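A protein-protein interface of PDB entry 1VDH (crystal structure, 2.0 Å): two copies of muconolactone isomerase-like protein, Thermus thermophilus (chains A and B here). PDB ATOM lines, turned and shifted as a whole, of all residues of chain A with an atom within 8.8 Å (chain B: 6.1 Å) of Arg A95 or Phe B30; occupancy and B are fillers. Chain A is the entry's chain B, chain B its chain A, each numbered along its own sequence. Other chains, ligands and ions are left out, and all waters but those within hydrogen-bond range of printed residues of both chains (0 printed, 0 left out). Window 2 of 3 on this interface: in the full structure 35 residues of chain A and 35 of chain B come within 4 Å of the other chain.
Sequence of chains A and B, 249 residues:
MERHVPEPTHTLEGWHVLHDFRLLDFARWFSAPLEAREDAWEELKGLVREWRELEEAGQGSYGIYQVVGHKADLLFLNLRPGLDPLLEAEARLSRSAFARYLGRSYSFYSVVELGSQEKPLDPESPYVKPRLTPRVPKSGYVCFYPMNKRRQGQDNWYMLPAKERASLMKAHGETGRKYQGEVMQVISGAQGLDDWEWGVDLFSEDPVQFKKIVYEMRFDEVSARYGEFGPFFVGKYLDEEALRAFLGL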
ATOM      1  N   ARG A  22      11.072  17.697  22.971  1.00  0.00           N
ATOM      2  CA  ARG A  22      12.065  18.758  22.925  1.00  0.00           C
ATOM      3  C   ARG A  22      11.859  19.669  21.730  1.00  0.00           C
ATOM      4  O   ARG A  22      11.277  19.268  20.722  1.00  0.00           O
ATOM      5  CB  ARG A  22      13.483  18.177  22.897  1.00  0.00           C
ATOM      6  CG  ARG A  22      13.723  17.157  23.996  1.00  0.00           C
ATOM      7  CD  ARG A  22      15.135  17.165  24.509  1.00  0.00           C
ATOM      8  NE  ARG A  22      15.336  16.035  25.409  1.00  0.00           N
ATOM      9  CZ  ARG A  22      16.381  15.884  26.213  1.00  0.00           C
ATOM     10  NH1 ARG A  22      17.340  16.800  26.244  1.00  0.00           N
ATOM     11  NH2 ARG A  22      16.468  14.803  26.979  1.00  0.00           N
ATOM     12  N   GLU A  43      26.753  10.676  16.294  1.00  0.00           N
ATOM     13  CA  GLU A  43      26.489  10.286  17.673  1.00  0.00           C
ATOM     14  C   GLU A  43      24.994  10.023  17.877  1.00  0.00           C
ATOM     15  O   GLU A  43      24.614   9.075  18.571  1.00  0.00           O
ATOM     16  CB  GLU A  43      26.962  11.378  18.638  1.00  0.00           C
ATOM     17  CG  GLU A  43      26.667  11.064  20.105  1.00  0.00           C
ATOM     18  CD  GLU A  43      27.010  12.207  21.036  1.00  0.00           C
ATOM     19  OE1 GLU A  43      27.404  11.930  22.187  1.00  0.00           O
ATOM     20  OE2 GLU A  43      26.888  13.380  20.625  1.00  0.00           O
ATOM     21  N   LEU A  47      23.176   6.474  19.017  1.00  0.00           N
ATOM     22  CA  LEU A  47      22.293   6.339  20.173  1.00  0.00           C
ATOM     23  C   LEU A  47      21.008   5.615  19.785  1.00  0.00           C
ATOM     24  O   LEU A  47      20.581   4.692  20.484  1.00  0.00           O
ATOM     25  CB  LEU A  47      21.955   7.718  20.753  1.00  0.00           C
ATOM     26  CG  LEU A  47      20.911   7.756  21.874  1.00  0.00           C
ATOM     27  CD1 LEU A  47      21.413   7.004  23.102  1.00  0.00           C
ATOM     28  CD2 LEU A  47      20.597   9.198  22.227  1.00  0.00           C
ATOM     29  N   GLU A  88      18.606   6.006  31.906  1.00  0.00           N
ATOM     30  CA  GLU A  88      19.813   5.834  31.103  1.00  0.00           C
ATOM     31  C   GLU A  88      19.639   6.454  29.716  1.00  0.00           C
ATOM     32  O   GLU A  88      20.433   7.295  29.310  1.00  0.00           O
ATOM     33  CB  GLU A  88      20.128   4.345  30.976  1.00  0.00           C
ATOM     34  CG  GLU A  88      21.367   4.013  30.167  1.00  0.00           C
ATOM     35  CD  GLU A  88      21.572   2.514  30.031  1.00  0.00           C
ATOM     36  OE1 GLU A  88      21.626   1.825  31.074  1.00  0.00           O
ATOM     37  OE2 GLU A  88      21.668   2.024  28.884  1.00  0.00           O
ATOM     38  N   ALA A  89      18.584   6.051  29.008  1.00  0.00           N
ATOM     39  CA  ALA A  89      18.297   6.561  27.667  1.00  0.00           C
ATOM     40  C   ALA A  89      18.141   8.076  27.661  1.00  0.00           C
ATOM     41  O   ALA A  89      18.604   8.757  26.746  1.00  0.00           O
ATOM     42  CB  ALA A  89      17.031   5.903  27.115  1.00  0.00           C
ATOM     43  N   GLU A  90      17.479   8.592  28.693  1.00  0.00           N
ATOM     44  CA  GLU A  90      17.232  10.023  28.842  1.00  0.00           C
ATOM     45  C   GLU A  90      18.530  10.797  29.108  1.00  0.00           C
ATOM     46  O   GLU A  90      18.794  11.824  28.479  1.00  0.00           O
ATOM     47  CB  GLU A  90      16.239  10.231  29.990  1.00  0.00           C
ATOM     48  CG  GLU A  90      15.917  11.665  30.336  1.00  0.00           C
ATOM     49  CD  GLU A  90      14.995  11.758  31.541  1.00  0.00           C
ATOM     50  OE1 GLU A  90      13.918  12.370  31.419  1.00  0.00           O
ATOM     51  OE2 GLU A  90      15.342  11.208  32.607  1.00  0.00           O
ATOM     52  N   ALA A  91      19.342  10.292  30.031  1.00  0.00           N
ATOM     53  CA  ALA A  91      20.608  10.942  30.373  1.00  0.00           C
ATOM     54  C   ALA A  91      21.563  10.962  29.180  1.00  0.00           C
ATOM     55  O   ALA A  91      22.216  11.975  28.912  1.00  0.00           O
ATOM     56  CB  ALA A  91      21.260  10.235  31.560  1.00  0.00           C
ATOM     57  N   ARG A  92      21.634   9.843  28.465  1.00  0.00           N
ATOM     58  CA  ARG A  92      22.508   9.734  27.300  1.00  0.00           C
ATOM     59  C   ARG A  92      22.090  10.680  26.179  1.00  0.00           C
ATOM     60  O   ARG A  92      22.941  11.257  25.503  1.00  0.00           O
ATOM     61  CB  ARG A  92      22.586   8.287  26.806  1.00  0.00           C
ATOM     62  CG  ARG A  92      23.226   7.351  27.826  1.00  0.00           C
ATOM     63  CD  ARG A  92      24.091   6.292  27.166  1.00  0.00           C
ATOM     64  NE  ARG A  92      23.491   4.962  27.208  1.00  0.00           N
ATOM     65  CZ  ARG A  92      24.084   3.862  26.754  1.00  0.00           C
ATOM     66  NH1 ARG A  92      25.298   3.928  26.221  1.00  0.00           N
ATOM     67  NH2 ARG A  92      23.463   2.694  26.833  1.00  0.00           N
ATOM     68  N   LEU A  93      20.785  10.861  25.995  1.00  0.00           N
ATOM     69  CA  LEU A  93      20.301  11.783  24.973  1.00  0.00           C
ATOM     70  C   LEU A  93      20.649  13.209  25.396  1.00  0.00           C
ATOM     71  O   LEU A  93      21.145  14.009  24.595  1.00  0.00           O
ATOM     72  CB  LEU A  93      18.781  11.664  24.791  1.00  0.00           C
ATOM     73  CG  LEU A  93      18.177  12.681  23.811  1.00  0.00           C
ATOM     74  CD1 LEU A  93      18.774  12.496  22.420  1.00  0.00           C
ATOM     75  CD2 LEU A  93      16.668  12.549  23.768  1.00  0.00           C
ATOM     76  N   SER A  94      20.401  13.511  26.666  1.00  0.00           N
ATOM     77  CA  SER A  94      20.663  14.837  27.211  1.00  0.00           C
ATOM     78  C   SER A  94      22.123  15.269  27.162  1.00  0.00           C
ATOM     79  O   SER A  94      22.411  16.457  27.038  1.00  0.00           O
ATOM     80  CB  SER A  94      20.127  14.941  28.638  1.00  0.00           C
ATOM     81  OG  SER A  94      18.716  15.068  28.637  1.00  0.00           O
ATOM     82  N   ARG A  95      23.044  14.315  27.240  1.00  0.00           N
ATOM     83  CA  ARG A  95      24.460  14.657  27.184  1.00  0.00           C
ATOM     84  C   ARG A  95      25.029  14.624  25.762  1.00  0.00           C
ATOM     85  O   ARG A  95      26.198  14.949  25.551  1.00  0.00           O
ATOM     86  CB  ARG A  95      25.286  13.762  28.115  1.00  0.00           C
ATOM     87  CG  ARG A  95      25.388  12.307  27.700  1.00  0.00           C
ATOM     88  CD  ARG A  95      26.504  11.612  28.467  1.00  0.00           C
ATOM     89  NE  ARG A  95      27.796  12.250  28.224  1.00  0.00           N
ATOM     90  CZ  ARG A  95      28.939  11.893  28.803  1.00  0.00           C
ATOM     91  NH1 ARG A  95      28.970  10.889  29.675  1.00  0.00           N
ATOM     92  NH2 ARG A  95      30.055  12.555  28.522  1.00  0.00           N
ATOM     93  N   SER A  96      24.199  14.259  24.786  1.00  0.00           N
ATOM     94  CA  SER A  96      24.654  14.201  23.395  1.00  0.00           C
ATOM     95  C   SER A  96      24.953  15.598  22.851  1.00  0.00           C
ATOM     96  O   SER A  96      24.429  16.595  23.352  1.00  0.00           O
ATOM     97  CB  SER A  96      23.599  13.536  22.504  1.00  0.00           C
ATOM     98  OG  SER A  96      22.490  14.397  22.282  1.00  0.00           O
ATOM     99  N   ALA A  97      25.796  15.662  21.825  1.00  0.00           N
ATOM    100  CA  ALA A  97      26.137  16.933  21.200  1.00  0.00           C
ATOM    101  C   ALA A  97      24.884  17.512  20.549  1.00  0.00           C
ATOM    102  O   ALA A  97      24.686  18.728  20.532  1.00  0.00           O
ATOM    103  CB  ALA A  97      27.232  16.734  20.150  1.00  0.00           C
ATOM    104  N   PHE A  98      24.033  16.637  20.018  1.00  0.00           N
ATOM    105  CA  PHE A  98      22.808  17.095  19.377  1.00  0.00           C
ATOM    106  C   PHE A  98      21.918  17.841  20.372  1.00  0.00           C
ATOM    107  O   PHE A  98      21.357  18.883  20.042  1.00  0.00           O
ATOM    108  CB  PHE A  98      22.039  15.922  18.757  1.00  0.00           C
ATOM    109  CG  PHE A  98      20.761  16.330  18.080  1.00  0.00           C
ATOM    110  CD1 PHE A  98      20.767  17.295  17.075  1.00  0.00           C
ATOM    111  CD2 PHE A  98      19.547  15.764  18.458  1.00  0.00           C
ATOM    112  CE1 PHE A  98      19.586  17.689  16.456  1.00  0.00           C
ATOM    113  CE2 PHE A  98      18.357  16.151  17.844  1.00  0.00           C
ATOM    114  CZ  PHE A  98      18.376  17.117  16.841  1.00  0.00           C
ATOM    115  N   ALA A  99      21.840  17.331  21.600  1.00  0.00           N
ATOM    116  CA  ALA A  99      21.021  17.944  22.649  1.00  0.00           C
ATOM    117  C   ALA A  99      21.428  19.377  22.984  1.00  0.00           C
ATOM    118  O   ALA A  99      20.647  20.118  23.585  1.00  0.00           O
ATOM    119  CB  ALA A  99      21.039  17.089  23.905  1.00  0.00           C
ATOM    120  N   ARG A 100      22.644  19.770  22.609  1.00  0.00           N
ATOM    121  CA  ARG A 100      23.094  21.138  22.873  1.00  0.00           C
ATOM    122  C   ARG A 100      22.204  22.109  22.097  1.00  0.00           C
ATOM    123  O   ARG A 100      22.091  23.283  22.449  1.00  0.00           O
ATOM    124  CB  ARG A 100      24.546  21.343  22.435  1.00  0.00           C
ATOM    125  CG  ARG A 100      25.560  20.416  23.081  1.00  0.00           C
ATOM    126  CD  ARG A 100      26.978  20.894  22.773  1.00  0.00           C
ATOM    127  NE  ARG A 100      27.985  19.834  22.857  1.00  0.00           N
ATOM    128  CZ  ARG A 100      28.267  19.124  23.950  1.00  0.00           C
ATOM    129  NH1 ARG A 100      27.617  19.338  25.089  1.00  0.00           N
ATOM    130  NH2 ARG A 100      29.230  18.209  23.905  1.00  0.00           N
ATOM    131  N   LEU B  24      19.848  20.284  35.409  1.00  0.00           N
ATOM    132  CA  LEU B  24      21.249  20.341  35.021  1.00  0.00           C
ATOM    133  C   LEU B  24      21.414  20.892  33.609  1.00  0.00           C
ATOM    134  O   LEU B  24      20.691  20.510  32.688  1.00  0.00           O
ATOM    135  CB  LEU B  24      21.878  18.948  35.113  1.00  0.00           C
ATOM    136  CG  LEU B  24      23.321  18.803  34.613  1.00  0.00           C
ATOM    137  CD1 LEU B  24      24.276  19.547  35.539  1.00  0.00           C
ATOM    138  CD2 LEU B  24      23.692  17.328  34.531  1.00  0.00           C
ATOM    139  N   ASP B  25      22.324  21.846  33.452  1.00  0.00           N
ATOM    140  CA  ASP B  25      22.598  22.391  32.133  1.00  0.00           C
ATOM    141  C   ASP B  25      23.615  21.407  31.546  1.00  0.00           C
ATOM    142  O   ASP B  25      24.827  21.591  31.689  1.00  0.00           O
ATOM    143  CB  ASP B  25      23.197  23.799  32.236  1.00  0.00           C
ATOM    144  CG  ASP B  25      23.357  24.476  30.874  1.00  0.00           C
ATOM    145  OD1 ASP B  25      23.402  23.777  29.838  1.00  0.00           O
ATOM    146  OD2 ASP B  25      23.447  25.719  30.842  1.00  0.00           O
ATOM    147  N   PHE B  26      23.102  20.340  30.934  1.00  0.00           N
ATOM    148  CA  PHE B  26      23.934  19.294  30.335  1.00  0.00           C
ATOM    149  C   PHE B  26      24.992  19.819  29.372  1.00  0.00           C
ATOM    150  O   PHE B  26      26.167  19.481  29.498  1.00  0.00           O
ATOM    151  CB  PHE B  26      23.066  18.253  29.614  1.00  0.00           C
ATOM    152  CG  PHE B  26      22.419  17.255  30.531  1.00  0.00           C
ATOM    153  CD1 PHE B  26      21.268  17.581  31.239  1.00  0.00           C
ATOM    154  CD2 PHE B  26      22.963  15.983  30.684  1.00  0.00           C
ATOM    155  CE1 PHE B  26      20.665  16.654  32.092  1.00  0.00           C
ATOM    156  CE2 PHE B  26      22.372  15.048  31.533  1.00  0.00           C
ATOM    157  CZ  PHE B  26      21.220  15.383  32.241  1.00  0.00           C
ATOM    158  N   ALA B  27      24.566  20.638  28.413  1.00  0.00           N
ATOM    159  CA  ALA B  27      25.464  21.210  27.418  1.00  0.00           C
ATOM    160  C   ALA B  27      26.655  21.931  28.041  1.00  0.00           C
ATOM    161  O   ALA B  27      27.799  21.696  27.650  1.00  0.00           O
ATOM    162  CB  ALA B  27      24.698  22.156  26.501  1.00  0.00           C
ATOM    163  N   ARG B  28      26.387  22.803  29.012  1.00  0.00           N
ATOM    164  CA  ARG B  28      27.450  23.551  29.676  1.00  0.00           C
ATOM    165  C   ARG B  28      28.345  22.687  30.552  1.00  0.00           C
ATOM    166  O   ARG B  28      29.562  22.849  30.545  1.00  0.00           O
ATOM    167  CB  ARG B  28      26.877  24.696  30.511  1.00  0.00           C
ATOM    168  CG  ARG B  28      26.633  25.980  29.735  1.00  0.00           C
ATOM    169  CD  ARG B  28      27.436  27.129  30.333  1.00  0.00           C
ATOM    170  NE  ARG B  28      27.097  27.373  31.737  1.00  0.00           N
ATOM    171  CZ  ARG B  28      27.959  27.793  32.660  1.00  0.00           C
ATOM    172  NH1 ARG B  28      27.549  27.988  33.905  1.00  0.00           N
ATOM    173  NH2 ARG B  28      29.231  28.011  32.347  1.00  0.00           N
ATOM    174  N   TRP B  29      27.741  21.773  31.305  1.00  0.00           N
ATOM    175  CA  TRP B  29      28.506  20.901  32.186  1.00  0.00           C
ATOM    176  C   TRP B  29      29.440  19.955  31.436  1.00  0.00           C
ATOM    177  O   TRP B  29      30.635  19.896  31.728  1.00  0.00           O
ATOM    178  CB  TRP B  29      27.574  20.088  33.086  1.00  0.00           C
ATOM    179  CG  TRP B  29      28.308  19.072  33.911  1.00  0.00           C
ATOM    180  CD1 TRP B  29      28.317  17.718  33.729  1.00  0.00           C
ATOM    181  CD2 TRP B  29      29.151  19.331  35.039  1.00  0.00           C
ATOM    182  NE1 TRP B  29      29.115  17.117  34.674  1.00  0.00           N
ATOM    183  CE2 TRP B  29      29.637  18.084  35.493  1.00  0.00           C
ATOM    184  CE3 TRP B  29      29.541  20.498  35.714  1.00  0.00           C
ATOM    185  CZ2 TRP B  29      30.493  17.968  36.594  1.00  0.00           C
ATOM    186  CZ3 TRP B  29      30.394  20.381  36.812  1.00  0.00           C
ATOM    187  CH2 TRP B  29      30.858  19.125  37.238  1.00  0.00           C
ATOM    188  N   PHE B  30      28.891  19.212  30.480  1.00  0.00           N
ATOM    189  CA  PHE B  30      29.679  18.252  29.715  1.00  0.00           C
ATOM    190  C   PHE B  30      30.651  18.862  28.704  1.00  0.00           C
ATOM    191  O   PHE B  30      31.504  18.159  28.161  1.00  0.00           O
ATOM    192  CB  PHE B  30      28.759  17.211  29.061  1.00  0.00           C
ATOM    193  CG  PHE B  30      28.105  16.282  30.055  1.00  0.00           C
ATOM    194  CD1 PHE B  30      26.831  16.550  30.549  1.00  0.00           C
ATOM    195  CD2 PHE B  30      28.781  15.158  30.527  1.00  0.00           C
ATOM    196  CE1 PHE B  30      26.241  15.717  31.502  1.00  0.00           C
ATOM    197  CE2 PHE B  30      28.200  14.318  31.480  1.00  0.00           C
ATOM    198  CZ  PHE B  30      26.928  14.600  31.970  1.00  0.00           C
ATOM    199  N   SER B  31      30.540  20.171  28.477  1.00  0.00           N
ATOM    200  CA  SER B  31      31.431  20.874  27.554  1.00  0.00           C
ATOM    201  C   SER B  31      32.473  21.692  28.313  1.00  0.00           C
ATOM    202  O   SER B  31      33.391  22.251  27.714  1.00  0.00           O
ATOM    203  CB  SER B  31      30.638  21.808  26.637  1.00  0.00           C
ATOM    204  OG  SER B  31      29.716  21.080  25.848  1.00  0.00           O
ATOM    205  N   ALA B  32      32.318  21.768  29.631  1.00  0.00           N
ATOM    206  CA  ALA B  32      33.234  22.523  30.479  1.00  0.00           C
ATOM    207  C   ALA B  32      34.585  21.826  30.592  1.00  0.00           C
ATOM    208  O   ALA B  32      34.671  20.604  30.453  1.00  0.00           O
ATOM    209  CB  ALA B  32      32.629  22.704  31.857  1.00  0.00           C
ATOM    210  N   ARG B  37      35.296  20.876  35.958  1.00  0.00           N
ATOM    211  CA  ARG B  37      34.356  19.859  36.404  1.00  0.00           C
ATOM    212  C   ARG B  37      34.869  19.165  37.663  1.00  0.00           C
ATOM    213  O   ARG B  37      34.130  19.015  38.640  1.00  0.00           O
ATOM    214  CB  ARG B  37      34.100  18.845  35.285  1.00  0.00           C
ATOM    215  CG  ARG B  37      33.442  19.455  34.048  1.00  0.00           C
ATOM    216  CD  ARG B  37      33.401  18.477  32.882  1.00  0.00           C
ATOM    217  NE  ARG B  37      32.652  17.269  33.217  1.00  0.00           N
ATOM    218  CZ  ARG B  37      32.617  16.170  32.467  1.00  0.00           C
ATOM    219  NH1 ARG B  37      31.910  15.124  32.866  1.00  0.00           N
ATOM    220  NH2 ARG B  37      33.278  16.119  31.313  1.00  0.00           N
ATOM    221  N   TYR B 101      26.025  25.367  37.014  1.00  0.00           N
ATOM    222  CA  TYR B 101      25.498  24.523  35.946  1.00  0.00           C
ATOM    223  C   TYR B 101      24.094  24.011  36.281  1.00  0.00           C
ATOM    224  O   TYR B 101      23.583  23.100  35.626  1.00  0.00           O
ATOM    225  CB  TYR B 101      26.441  23.338  35.709  1.00  0.00           C
ATOM    226  CG  TYR B 101      27.867  23.758  35.434  1.00  0.00           C
ATOM    227  CD1 TYR B 101      28.306  23.988  34.131  1.00  0.00           C
ATOM    228  CD2 TYR B 101      28.771  23.947  36.480  1.00  0.00           C
ATOM    229  CE1 TYR B 101      29.613  24.399  33.874  1.00  0.00           C
ATOM    230  CE2 TYR B 101      30.079  24.360  36.233  1.00  0.00           C
ATOM    231  CZ  TYR B 101      30.492  24.584  34.929  1.00  0.00           C
ATOM    232  OH  TYR B 101      31.782  24.993  34.674  1.00  0.00           O
ATOM    233  N   ALA B 245      29.136   9.148  38.504  1.00  0.00           N
ATOM    234  CA  ALA B 245      28.891   8.533  37.198  1.00  0.00           C
ATOM    235  C   ALA B 245      27.898   9.345  36.368  1.00  0.00           C
ATOM    236  O   ALA B 245      28.078   9.519  35.163  1.00  0.00           O
ATOM    237  CB  ALA B 245      28.383   7.101  37.372  1.00  0.00           C
ATOM    238  N   PHE B 246      26.845   9.823  37.026  1.00  0.00           N
ATOM    239  CA  PHE B 246      25.814  10.633  36.381  1.00  0.00           C
ATOM    240  C   PHE B 246      26.427  11.906  35.778  1.00  0.00           C
ATOM    241  O   PHE B 246      26.052  12.334  34.682  1.00  0.00           O
ATOM    242  CB  PHE B 246      24.735  11.006  37.408  1.00  0.00           C
ATOM    243  CG  PHE B 246      23.721  11.991  36.896  1.00  0.00           C
ATOM    244  CD1 PHE B 246      22.790  11.614  35.936  1.00  0.00           C
ATOM    245  CD2 PHE B 246      23.706  13.301  37.369  1.00  0.00           C
ATOM    246  CE1 PHE B 246      21.851  12.531  35.453  1.00  0.00           C
ATOM    247  CE2 PHE B 246      22.774  14.220  36.893  1.00  0.00           C
ATOM    248  CZ  PHE B 246      21.845  13.833  35.932  1.00  0.00           C
ATOM    249  N   LEU B 247      27.386  12.489  36.494  1.00  0.00           N
ATOM    250  CA  LEU B 247      28.056  13.705  36.043  1.00  0.00           C
ATOM    251  C   LEU B 247      29.191  13.424  35.058  1.00  0.00           C
ATOM    252  O   LEU B 247      29.901  14.340  34.634  1.00  0.00           O
ATOM    253  CB  LEU B 247      28.564  14.500  37.250  1.00  0.00           C
ATOM    254  CG  LEU B 247      27.453  14.914  38.223  1.00  0.00           C
ATOM    255  CD1 LEU B 247      28.036  15.599  39.457  1.00  0.00           C
ATOM    256  CD2 LEU B 247      26.454  15.825  37.513  1.00  0.00           C
ATOM    257  N   GLY B 248      29.348  12.154  34.691  1.00  0.00           N
ATOM    258  CA  GLY B 248      30.379  11.764  33.745  1.00  0.00           C
ATOM    259  C   GLY B 248      31.798  11.824  34.279  1.00  0.00           C
ATOM    260  O   GLY B 248      32.746  12.010  33.516  1.00  0.00           O
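The guanidinium group (NH1) of Arg A100 is in hydrogen-bond range of the side-chain hydroxyl (OG) of Ser B31 (2.8 Å).
O of Ala B27 sits at hydrogen-bond distance from NH1 of Arg A100, at 3.5 Å.
O of Ala B27 lies within hydrogen-bond range of OG of Ser B31.
The guanidinium group (NH2) of Arg A22 lies within hydrogen-bond range of the side-chain hydroxyl (OG) of Ser A94, 2.8 Å away.
The side-chain hydroxyl of Ser A94 sits at hydrogen-bond distance from the backbone carbonyl oxygen of Glu A90, 3.2 Å away.
Among the printed residues, merely in contact across the chains: Ser A94 with Phe B26 (3.2 Å), Arg A95 with Phe B26 (3.8 Å) and Arg A95 with Phe B30 (3.5 Å).
Of the printed residues of chain A, Phe B30 touches Arg A95.
Of the printed residues of chain A, Phe B26 touches Ser A94 (3.2 Å) and Arg A95 (3.8 Å).
Of the printed residues of chain B, Ser A94 touches Phe B26.
Of the printed residues of chain B, Arg A100 touches Ala B27 and Ser B31.
Of the printed residues of chain A, Ala B27 touches Arg A100 (3.5 Å).
Phe B246 touches none of the printed residues of chain A.
The nearest residue of chain B that does not touch Arg A95 is Gly B248 (4.4 Å).
The nearest residue of chain A that does not touch Phe B30 is Arg A100 (4.6 Å).
The nearest printed residue of chain A that does not touch Phe B26 is Ala A91 (4.04 Å).
Of the 16 printed residues of chain A, 3 touch a printed residue of chain B.
Along chain A the printed residues that touch a printed residue of chain B span positions 94 to 100.
Of the 15 printed residues of chain B, 4 touch a printed residue of chain A.
Along chain B the printed residues that touch a printed residue of chain A span positions 26 to 31.
Among the printed residues, 5 pairs touch across the chains.
Among the printed residues, no Asp or Glu carboxylate lies within 4 Å of a Lys or Arg side-chain nitrogen of the other chain.
No position is printed for both chains.
Of the 5 pairs that touch across the chains among the printed residues, none has its exchanged pair printed and touching as well.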
